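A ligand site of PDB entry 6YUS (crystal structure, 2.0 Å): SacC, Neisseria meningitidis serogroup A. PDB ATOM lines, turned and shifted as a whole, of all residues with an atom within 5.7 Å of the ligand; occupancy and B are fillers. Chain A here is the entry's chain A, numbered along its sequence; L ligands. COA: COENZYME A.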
ATOM      1  N   ILE A  11     -31.296  31.915  34.393  1.00  0.00           N
ATOM      2  CA  ILE A  11     -31.457  30.491  34.093  1.00  0.00           C
ATOM      3  C   ILE A  11     -30.517  29.717  35.008  1.00  0.00           C
ATOM      4  O   ILE A  11     -29.292  29.867  34.916  1.00  0.00           O
ATOM      5  CB  ILE A  11     -31.146  30.188  32.624  1.00  0.00           C
ATOM      6  CG1 ILE A  11     -32.230  30.730  31.689  1.00  0.00           C
ATOM      7  CG2 ILE A  11     -30.981  28.687  32.416  1.00  0.00           C
ATOM      8  CD1 ILE A  11     -32.217  32.239  31.511  1.00  0.00           C
ATOM      9  N   LEU A  12     -31.076  28.861  35.858  1.00  0.00           N
ATOM     10  CA  LEU A  12     -30.293  28.206  36.893  1.00  0.00           C
ATOM     11  C   LEU A  12     -29.490  29.254  37.634  1.00  0.00           C
ATOM     12  O   LEU A  12     -30.009  30.342  37.920  1.00  0.00           O
ATOM     13  CB  LEU A  12     -29.418  27.105  36.293  1.00  0.00           C
ATOM     14  CG  LEU A  12     -30.243  25.947  35.701  1.00  0.00           C
ATOM     15  CD1 LEU A  12     -29.382  24.760  35.317  1.00  0.00           C
ATOM     16  CD2 LEU A  12     -31.327  25.510  36.708  1.00  0.00           C
ATOM     17  N   GLU A  16     -28.814  36.178  32.451  1.00  0.00           N
ATOM     18  CA  GLU A  16     -28.828  36.290  31.010  1.00  0.00           C
ATOM     19  C   GLU A  16     -28.574  37.737  30.599  1.00  0.00           C
ATOM     20  O   GLU A  16     -29.033  38.666  31.265  1.00  0.00           O
ATOM     21  CB  GLU A  16     -30.161  35.811  30.423  1.00  0.00           C
ATOM     22  CG  GLU A  16     -30.279  35.979  28.917  1.00  0.00           C
ATOM     23  CD  GLU A  16     -31.647  35.571  28.410  1.00  0.00           C
ATOM     24  OE1 GLU A  16     -32.647  36.234  28.757  1.00  0.00           O
ATOM     25  OE2 GLU A  16     -31.733  34.586  27.658  1.00  0.00           O
ATOM     26  N   ALA A  39     -28.998  24.384  20.382  1.00  0.00           N
ATOM     27  CA  ALA A  39     -29.438  23.546  19.277  1.00  0.00           C
ATOM     28  C   ALA A  39     -30.864  23.927  18.889  1.00  0.00           C
ATOM     29  O   ALA A  39     -31.521  24.743  19.543  1.00  0.00           O
ATOM     30  CB  ALA A  39     -29.336  22.054  19.648  1.00  0.00           C
ATOM     31  N   PHE A  40     -31.344  23.311  17.820  1.00  0.00           N
ATOM     32  CA  PHE A  40     -32.606  23.677  17.196  1.00  0.00           C
ATOM     33  C   PHE A  40     -33.756  23.140  18.045  1.00  0.00           C
ATOM     34  O   PHE A  40     -33.857  21.912  18.221  1.00  0.00           O
ATOM     35  CB  PHE A  40     -32.598  23.090  15.784  1.00  0.00           C
ATOM     36  CG  PHE A  40     -33.587  23.690  14.808  1.00  0.00           C
ATOM     37  CD1 PHE A  40     -33.301  23.642  13.440  1.00  0.00           C
ATOM     38  CD2 PHE A  40     -34.801  24.230  15.210  1.00  0.00           C
ATOM     39  CE1 PHE A  40     -34.197  24.111  12.485  1.00  0.00           C
ATOM     40  CE2 PHE A  40     -35.711  24.716  14.253  1.00  0.00           C
ATOM     41  CZ  PHE A  40     -35.420  24.658  12.896  1.00  0.00           C
ATOM     42  N   ALA A  46     -39.168  27.276  23.022  1.00  0.00           N
ATOM     43  CA  ALA A  46     -38.238  28.390  22.937  1.00  0.00           C
ATOM     44  C   ALA A  46     -36.808  27.878  22.912  1.00  0.00           C
ATOM     45  O   ALA A  46     -36.498  26.782  23.395  1.00  0.00           O
ATOM     46  CB  ALA A  46     -38.407  29.347  24.117  1.00  0.00           C
ATOM     47  N   GLN A  47     -35.921  28.691  22.332  1.00  0.00           N
ATOM     48  CA  GLN A  47     -34.512  28.344  22.293  1.00  0.00           C
ATOM     49  C   GLN A  47     -33.976  28.213  23.706  1.00  0.00           C
ATOM     50  O   GLN A  47     -34.152  29.117  24.538  1.00  0.00           O
ATOM     51  CB  GLN A  47     -33.728  29.421  21.530  1.00  0.00           C
ATOM     52  CG  GLN A  47     -34.204  29.678  20.095  1.00  0.00           C
ATOM     53  CD  GLN A  47     -33.287  30.664  19.362  1.00  0.00           C
ATOM     54  OE1 GLN A  47     -32.098  30.707  19.625  1.00  0.00           O
ATOM     55  NE2 GLN A  47     -33.853  31.456  18.463  1.00  0.00           N
ATOM     56  N   LYS A  48     -33.306  27.095  23.979  1.00  0.00           N
ATOM     57  CA  LYS A  48     -32.715  26.840  25.281  1.00  0.00           C
ATOM     58  C   LYS A  48     -31.192  26.848  25.196  1.00  0.00           C
ATOM     59  O   LYS A  48     -30.601  26.483  24.180  1.00  0.00           O
ATOM     60  CB  LYS A  48     -33.190  25.496  25.852  1.00  0.00           C
ATOM     61  CG  LYS A  48     -34.686  25.441  26.202  1.00  0.00           C
ATOM     62  CD  LYS A  48     -35.081  24.080  26.770  1.00  0.00           C
ATOM     63  CE  LYS A  48     -36.605  24.005  26.993  1.00  0.00           C
ATOM     64  NZ  LYS A  48     -37.151  25.343  27.360  1.00  0.00           N
ATOM     65  N   TYR A  49     -30.561  27.295  26.289  1.00  0.00           N
ATOM     66  CA  TYR A  49     -29.133  27.094  26.494  1.00  0.00           C
ATOM     67  C   TYR A  49     -28.847  25.613  26.765  1.00  0.00           C
ATOM     68  O   TYR A  49     -29.550  24.962  27.521  1.00  0.00           O
ATOM     69  CB  TYR A  49     -28.661  27.956  27.663  1.00  0.00           C
ATOM     70  CG  TYR A  49     -28.922  29.424  27.433  1.00  0.00           C
ATOM     71  CD1 TYR A  49     -28.040  30.194  26.678  1.00  0.00           C
ATOM     72  CD2 TYR A  49     -30.056  30.043  27.934  1.00  0.00           C
ATOM     73  CE1 TYR A  49     -28.268  31.520  26.446  1.00  0.00           C
ATOM     74  CE2 TYR A  49     -30.298  31.387  27.699  1.00  0.00           C
ATOM     75  CZ  TYR A  49     -29.402  32.118  26.952  1.00  0.00           C
ATOM     76  OH  TYR A  49     -29.626  33.450  26.708  1.00  0.00           O
ATOM     77  N   ASN A  50     -27.789  25.083  26.159  1.00  0.00           N
ATOM     78  CA  ASN A  50     -27.505  23.658  26.243  1.00  0.00           C
ATOM     79  C   ASN A  50     -26.233  23.391  27.050  1.00  0.00           C
ATOM     80  O   ASN A  50     -25.247  24.133  26.951  1.00  0.00           O
ATOM     81  CB  ASN A  50     -27.406  23.055  24.848  1.00  0.00           C
ATOM     82  CG  ASN A  50     -28.745  23.091  24.086  1.00  0.00           C
ATOM     83  OD1 ASN A  50     -28.789  23.125  22.860  1.00  0.00           O
ATOM     84  ND2 ASN A  50     -29.835  23.116  24.838  1.00  0.00           N
ATOM     85  N   TYR A  51     -26.280  22.355  27.888  1.00  0.00           N
ATOM     86  CA  TYR A  51     -25.112  21.817  28.599  1.00  0.00           C
ATOM     87  C   TYR A  51     -24.640  22.747  29.722  1.00  0.00           C
ATOM     88  O   TYR A  51     -23.448  22.867  29.979  1.00  0.00           O
ATOM     89  CB  TYR A  51     -23.980  21.495  27.612  1.00  0.00           C
ATOM     90  CG  TYR A  51     -24.480  20.621  26.479  1.00  0.00           C
ATOM     91  CD1 TYR A  51     -25.216  19.460  26.743  1.00  0.00           C
ATOM     92  CD2 TYR A  51     -24.288  20.985  25.161  1.00  0.00           C
ATOM     93  CE1 TYR A  51     -25.721  18.675  25.724  1.00  0.00           C
ATOM     94  CE2 TYR A  51     -24.797  20.192  24.103  1.00  0.00           C
ATOM     95  CZ  TYR A  51     -25.511  19.030  24.407  1.00  0.00           C
ATOM     96  OH  TYR A  51     -26.028  18.243  23.400  1.00  0.00           O
ATOM     97  N   ILE A  52     -25.594  23.382  30.400  1.00  0.00           N
ATOM     98  CA  ILE A  52     -25.319  24.136  31.619  1.00  0.00           C
ATOM     99  C   ILE A  52     -25.003  23.203  32.784  1.00  0.00           C
ATOM    100  O   ILE A  52     -24.031  23.395  33.526  1.00  0.00           O
ATOM    101  CB  ILE A  52     -26.503  25.039  31.980  1.00  0.00           C
ATOM    102  CG1 ILE A  52     -26.833  26.039  30.872  1.00  0.00           C
ATOM    103  CG2 ILE A  52     -26.253  25.722  33.319  1.00  0.00           C
ATOM    104  CD1 ILE A  52     -28.160  26.732  31.126  1.00  0.00           C
ATOM    105  N   LYS A  53     -25.877  22.215  33.022  1.00  0.00           N
ATOM    106  CA  LYS A  53     -25.708  21.392  34.206  1.00  0.00           C
ATOM    107  C   LYS A  53     -24.383  20.637  34.192  1.00  0.00           C
ATOM    108  O   LYS A  53     -23.816  20.367  35.263  1.00  0.00           O
ATOM    109  CB  LYS A  53     -26.897  20.457  34.324  1.00  0.00           C
ATOM    110  CG  LYS A  53     -28.204  21.245  34.237  1.00  0.00           C
ATOM    111  CD  LYS A  53     -29.391  20.550  34.887  1.00  0.00           C
ATOM    112  CE  LYS A  53     -29.714  19.278  34.176  1.00  0.00           C
ATOM    113  NZ  LYS A  53     -31.058  19.330  33.505  1.00  0.00           N
ATOM    114  N   ASP A  54     -23.835  20.381  32.991  1.00  0.00           N
ATOM    115  CA  ASP A  54     -22.534  19.735  32.873  1.00  0.00           C
ATOM    116  C   ASP A  54     -21.434  20.521  33.596  1.00  0.00           C
ATOM    117  O   ASP A  54     -20.464  19.928  34.078  1.00  0.00           O
ATOM    118  CB  ASP A  54     -22.180  19.546  31.396  1.00  0.00           C
ATOM    119  CG  ASP A  54     -23.069  18.528  30.696  1.00  0.00           C
ATOM    120  OD1 ASP A  54     -24.107  18.926  30.129  1.00  0.00           O
ATOM    121  OD2 ASP A  54     -22.724  17.321  30.728  1.00  0.00           O
ATOM    122  N   LEU A  66     -27.650  31.753  22.688  1.00  0.00           N
ATOM    123  CA  LEU A  66     -28.784  31.447  21.821  1.00  0.00           C
ATOM    124  C   LEU A  66     -28.518  31.914  20.381  1.00  0.00           C
ATOM    125  O   LEU A  66     -27.548  32.635  20.082  1.00  0.00           O
ATOM    126  CB  LEU A  66     -30.056  32.104  22.345  1.00  0.00           C
ATOM    127  CG  LEU A  66     -30.462  31.714  23.779  1.00  0.00           C
ATOM    128  CD1 LEU A  66     -31.759  32.363  24.225  1.00  0.00           C
ATOM    129  CD2 LEU A  66     -30.518  30.207  23.930  1.00  0.00           C
ATOM    130  N   SER A 113     -24.429  20.394  19.982  1.00  0.00           N
ATOM    131  CA  SER A 113     -24.969  19.269  19.215  1.00  0.00           C
ATOM    132  C   SER A 113     -25.912  19.771  18.124  1.00  0.00           C
ATOM    133  O   SER A 113     -26.582  20.793  18.314  1.00  0.00           O
ATOM    134  CB  SER A 113     -25.732  18.336  20.130  1.00  0.00           C
ATOM    135  OG  SER A 113     -26.646  19.128  20.873  1.00  0.00           O
ATOM    136  N   OAS A 114     -25.979  19.065  16.991  1.00  0.00           N
ATOM    137  CA  OAS A 114     -26.954  19.435  15.992  1.00  0.00           C
ATOM    138  CB  OAS A 114     -28.391  19.375  16.565  1.00  0.00           C
ATOM    139  OG  OAS A 114     -29.281  19.197  15.455  1.00  0.00           O
ATOM    140  C   OAS A 114     -26.609  20.857  15.477  1.00  0.00           C
ATOM    141  O   OAS A 114     -25.457  21.191  15.125  1.00  0.00           O
ATOM    142  C2A OAS A 114     -30.787  20.154  14.022  1.00  0.00           C
ATOM    143  C1A OAS A 114     -30.320  20.084  15.406  1.00  0.00           C
ATOM    144  OAC OAS A 114     -30.427  20.971  16.257  1.00  0.00           O
ATOM    145  N   ASN A 135     -21.419  17.189  18.355  1.00  0.00           N
ATOM    146  CA  ASN A 135     -22.094  15.960  17.941  1.00  0.00           C
ATOM    147  C   ASN A 135     -23.008  16.242  16.762  1.00  0.00           C
ATOM    148  O   ASN A 135     -23.773  17.218  16.775  1.00  0.00           O
ATOM    149  CB  ASN A 135     -22.902  15.341  19.068  1.00  0.00           C
ATOM    150  CG  ASN A 135     -23.603  14.102  18.658  1.00  0.00           C
ATOM    151  OD1 ASN A 135     -22.984  13.025  18.598  1.00  0.00           O
ATOM    152  ND2 ASN A 135     -24.904  14.216  18.349  1.00  0.00           N
ATOM    153  N   TYR A 144     -31.288  20.806   5.404  1.00  0.00           N
ATOM    154  CA  TYR A 144     -31.804  20.389   6.709  1.00  0.00           C
ATOM    155  C   TYR A 144     -32.881  21.338   7.225  1.00  0.00           C
ATOM    156  O   TYR A 144     -33.924  20.894   7.706  1.00  0.00           O
ATOM    157  CB  TYR A 144     -30.687  20.273   7.763  1.00  0.00           C
ATOM    158  CG  TYR A 144     -31.280  19.740   9.048  1.00  0.00           C
ATOM    159  CD1 TYR A 144     -31.648  18.390   9.180  1.00  0.00           C
ATOM    160  CD2 TYR A 144     -31.595  20.595  10.088  1.00  0.00           C
ATOM    161  CE1 TYR A 144     -32.239  17.902  10.332  1.00  0.00           C
ATOM    162  CE2 TYR A 144     -32.204  20.115  11.239  1.00  0.00           C
ATOM    163  CZ  TYR A 144     -32.509  18.781  11.373  1.00  0.00           C
ATOM    164  OH  TYR A 144     -33.090  18.314  12.540  1.00  0.00           O
ATOM    165  N   ARG A 148     -37.405  21.262   8.772  1.00  0.00           N
ATOM    166  CA  ARG A 148     -37.840  21.647  10.110  1.00  0.00           C
ATOM    167  C   ARG A 148     -38.768  22.840  10.129  1.00  0.00           C
ATOM    168  O   ARG A 148     -39.643  22.905  10.998  1.00  0.00           O
ATOM    169  CB  ARG A 148     -36.632  21.971  11.008  1.00  0.00           C
ATOM    170  CG  ARG A 148     -35.826  20.753  11.457  1.00  0.00           C
ATOM    171  CD  ARG A 148     -36.665  19.698  12.158  1.00  0.00           C
ATOM    172  NE  ARG A 148     -37.183  20.093  13.469  1.00  0.00           N
ATOM    173  CZ  ARG A 148     -36.449  20.174  14.573  1.00  0.00           C
ATOM    174  NH1 ARG A 148     -35.152  19.921  14.553  1.00  0.00           N
ATOM    175  NH2 ARG A 148     -37.034  20.513  15.717  1.00  0.00           N
ATOM    176  N   ASN A 230     -31.496  10.976  22.230  1.00  0.00           N
ATOM    177  CA  ASN A 230     -30.887  11.385  23.487  1.00  0.00           C
ATOM    178  C   ASN A 230     -29.905  10.353  24.014  1.00  0.00           C
ATOM    179  O   ASN A 230     -29.143  10.649  24.944  1.00  0.00           O
ATOM    180  CB  ASN A 230     -31.987  11.637  24.528  1.00  0.00           C
ATOM    181  CG  ASN A 230     -33.145  12.434  23.955  1.00  0.00           C
ATOM    182  OD1 ASN A 230     -33.646  12.121  22.873  1.00  0.00           O
ATOM    183  ND2 ASN A 230     -33.574  13.455  24.679  1.00  0.00           N
ATOM    184  N   ILE A 233     -26.865  11.813  22.633  1.00  0.00           N
ATOM    185  CA  ILE A 233     -26.535  13.030  23.365  1.00  0.00           C
ATOM    186  C   ILE A 233     -25.821  12.685  24.677  1.00  0.00           C
ATOM    187  O   ILE A 233     -24.839  13.323  25.052  1.00  0.00           O
ATOM    188  CB  ILE A 233     -27.806  13.864  23.604  1.00  0.00           C
ATOM    189  CG1 ILE A 233     -28.338  14.427  22.281  1.00  0.00           C
ATOM    190  CG2 ILE A 233     -27.545  14.996  24.587  1.00  0.00           C
ATOM    191  CD1 ILE A 233     -27.295  15.303  21.531  1.00  0.00           C
ATOM    192  N   ARG A 237     -22.151  13.981  25.766  1.00  0.00           N
ATOM    193  CA  ARG A 237     -21.820  14.599  27.052  1.00  0.00           C
ATOM    194  C   ARG A 237     -20.669  13.885  27.751  1.00  0.00           C
ATOM    195  O   ARG A 237     -19.775  14.535  28.316  1.00  0.00           O
ATOM    196  CB  ARG A 237     -23.050  14.594  27.955  1.00  0.00           C
ATOM    197  CG  ARG A 237     -24.192  15.427  27.423  1.00  0.00           C
ATOM    198  CD  ARG A 237     -24.778  16.229  28.548  1.00  0.00           C
ATOM    199  NE  ARG A 237     -26.216  16.075  28.668  1.00  0.00           N
ATOM    200  CZ  ARG A 237     -26.951  16.739  29.558  1.00  0.00           C
ATOM    201  NH1 ARG A 237     -26.371  17.624  30.354  1.00  0.00           N
ATOM    202  NH2 ARG A 237     -28.271  16.506  29.635  1.00  0.00           N
HETATM  203  N1A COA L   1     -35.223  30.188  29.711  1.00  0.00           N
HETATM  204  C2A COA L   1     -35.449  29.534  30.860  1.00  0.00           C
HETATM  205  N3A COA L   1     -34.752  28.382  31.138  1.00  0.00           N
HETATM  206  C4A COA L   1     -33.830  27.900  30.244  1.00  0.00           C
HETATM  207  C5A COA L   1     -33.599  28.543  29.108  1.00  0.00           C
HETATM  208  C6A COA L   1     -34.306  29.719  28.815  1.00  0.00           C
HETATM  209  N6A COA L   1     -34.335  30.720  27.652  1.00  0.00           N
HETATM  210  N7A COA L   1     -32.649  27.851  28.423  1.00  0.00           N
HETATM  211  C8A COA L   1     -32.309  26.785  29.163  1.00  0.00           C
HETATM  212  N9A COA L   1     -33.033  26.809  30.286  1.00  0.00           N
HETATM  213  C1B COA L   1     -33.001  25.876  31.320  1.00  0.00           C
HETATM  214  C2B COA L   1     -33.706  24.797  30.989  1.00  0.00           C
HETATM  215  O2B COA L   1     -35.124  24.976  31.332  1.00  0.00           O
HETATM  216  C3B COA L   1     -33.044  23.691  31.825  1.00  0.00           C
HETATM  217  O3B COA L   1     -33.390  23.842  33.124  1.00  0.00           O
HETATM  218  P3B COA L   1     -34.333  22.713  33.963  1.00  0.00           P
HETATM  219  O7A COA L   1     -34.521  21.465  33.154  1.00  0.00           O
HETATM  220  O8A COA L   1     -33.682  22.373  35.227  1.00  0.00           O
HETATM  221  O9A COA L   1     -35.635  23.343  34.239  1.00  0.00           O
HETATM  222  C4B COA L   1     -31.515  24.036  31.685  1.00  0.00           C
HETATM  223  O4B COA L   1     -31.461  25.327  31.490  1.00  0.00           O
HETATM  224  C5B COA L   1     -30.849  23.307  30.507  1.00  0.00           C
HETATM  225  O5B COA L   1     -30.306  22.124  31.083  1.00  0.00           O
HETATM  226  P1A COA L   1     -28.954  21.252  30.363  1.00  0.00           P
HETATM  227  O1A COA L   1     -27.659  21.770  30.985  1.00  0.00           O
HETATM  228  O2A COA L   1     -28.970  21.423  28.796  1.00  0.00           O
HETATM  229  O3A COA L   1     -29.010  19.709  30.768  1.00  0.00           O
HETATM  230  P2A COA L   1     -30.327  18.680  30.599  1.00  0.00           P
HETATM  231  O4A COA L   1     -30.097  17.506  31.506  1.00  0.00           O
HETATM  232  O5A COA L   1     -31.603  19.434  30.917  1.00  0.00           O
HETATM  233  O6A COA L   1     -30.357  18.096  28.994  1.00  0.00           O
HETATM  234  CBP COA L   1     -31.054  18.342  26.799  1.00  0.00           C
HETATM  235  CCP COA L   1     -31.424  18.541  28.244  1.00  0.00           C
HETATM  236  CDP COA L   1     -32.278  17.853  26.071  1.00  0.00           C
HETATM  237  CEP COA L   1     -29.906  17.280  26.682  1.00  0.00           C
HETATM  238  CAP COA L   1     -30.551  19.725  26.299  1.00  0.00           C
HETATM  239  OAP COA L   1     -29.140  19.862  26.544  1.00  0.00           O
HETATM  240  C9P COA L   1     -30.801  19.826  24.818  1.00  0.00           C
HETATM  241  O9P COA L   1     -31.855  20.270  24.396  1.00  0.00           O
HETATM  242  N8P COA L   1     -29.725  19.392  23.912  1.00  0.00           N
HETATM  243  C7P COA L   1     -29.947  19.484  22.492  1.00  0.00           C
HETATM  244  C6P COA L   1     -29.431  18.115  21.816  1.00  0.00           C
HETATM  245  C5P COA L   1     -29.842  18.202  20.290  1.00  0.00           C
HETATM  246  O5P COA L   1     -29.109  17.795  19.467  1.00  0.00           O
HETATM  247  N4P COA L   1     -31.131  18.807  19.965  1.00  0.00           N
HETATM  248  C3P COA L   1     -31.589  18.917  18.529  1.00  0.00           C
HETATM  249  C2P COA L   1     -32.052  17.523  18.052  1.00  0.00           C
HETATM  250  S1P COA L   1     -32.468  17.568  16.310  1.00  0.00           S
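An oxygen (O4A) of the ligand lies within salt-bridge range of the guanidinium group (NH2) of Arg 237.
An oxygen (O5A) of the ligand is in salt-bridge range of the side-chain amino group (NZ) of Lys 53 (2.6 Å).
The side-chain hydroxyl of Ser 113 lies close to an oxygen (O5P) of the ligand, at 3.1 Å.
O1A of the ligand sits at hydrogen-bond distance from N of Ile 52 (2.7 Å).
O2A of the ligand is in hydrogen-bond range of N of Tyr 51 (3.0 Å).
N of Tyr 49 sits at hydrogen-bond distance from N7A of the ligand (3.0 Å).
A sulfur (S1P) of the ligand sits close to OG of OAS 114, 3.7 Å away.
O1A of the ligand sits at hydrogen-bond distance from N of Lys 53 (2.7 Å).
OAC of OAS 114 sits at hydrogen-bond distance from N of Phe 40, at 3.0 Å.
OG of Ser 113 is in hydrogen-bond range of OH of Tyr 51, at 2.7 Å.
OD1 of Asn 50 sits at hydrogen-bond distance from N of Ala 39, at 2.8 Å.
N of OAS 114 sits at hydrogen-bond distance from the backbone carbonyl oxygen of Asn 135 (2.9 Å).
OH of Tyr 49 sits at hydrogen-bond distance from OE2 of Glu 16 (2.6 Å).
The guanidinium group (NH1) of Arg 148 is in hydrogen-bond range of the side-chain hydroxyl (OH) of Tyr 144 (3.3 Å).
NH1 of Arg 237 is in salt-bridge range of OD1 of Asp 54, at 2.6 Å.
CG1 of Ile 11 touches N3A of the ligand, at 3.5 Å.
Ala 39 touches the ligand.
Phe 40 touches the ligand.
Gln 47 touches the ligand (O to N6A, 3.5 Å).
Lys 48 touches the ligand (CA to N7A, 3.3 Å).
Asn 50 touches the ligand.
Tyr 144 touches the ligand (OH to S1P, 3.9 Å).
Arg 148 touches the ligand (NH1 to S1P, 3.98 Å).
Ile 233 touches the ligand (CD1 to C6P, 3.5 Å).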
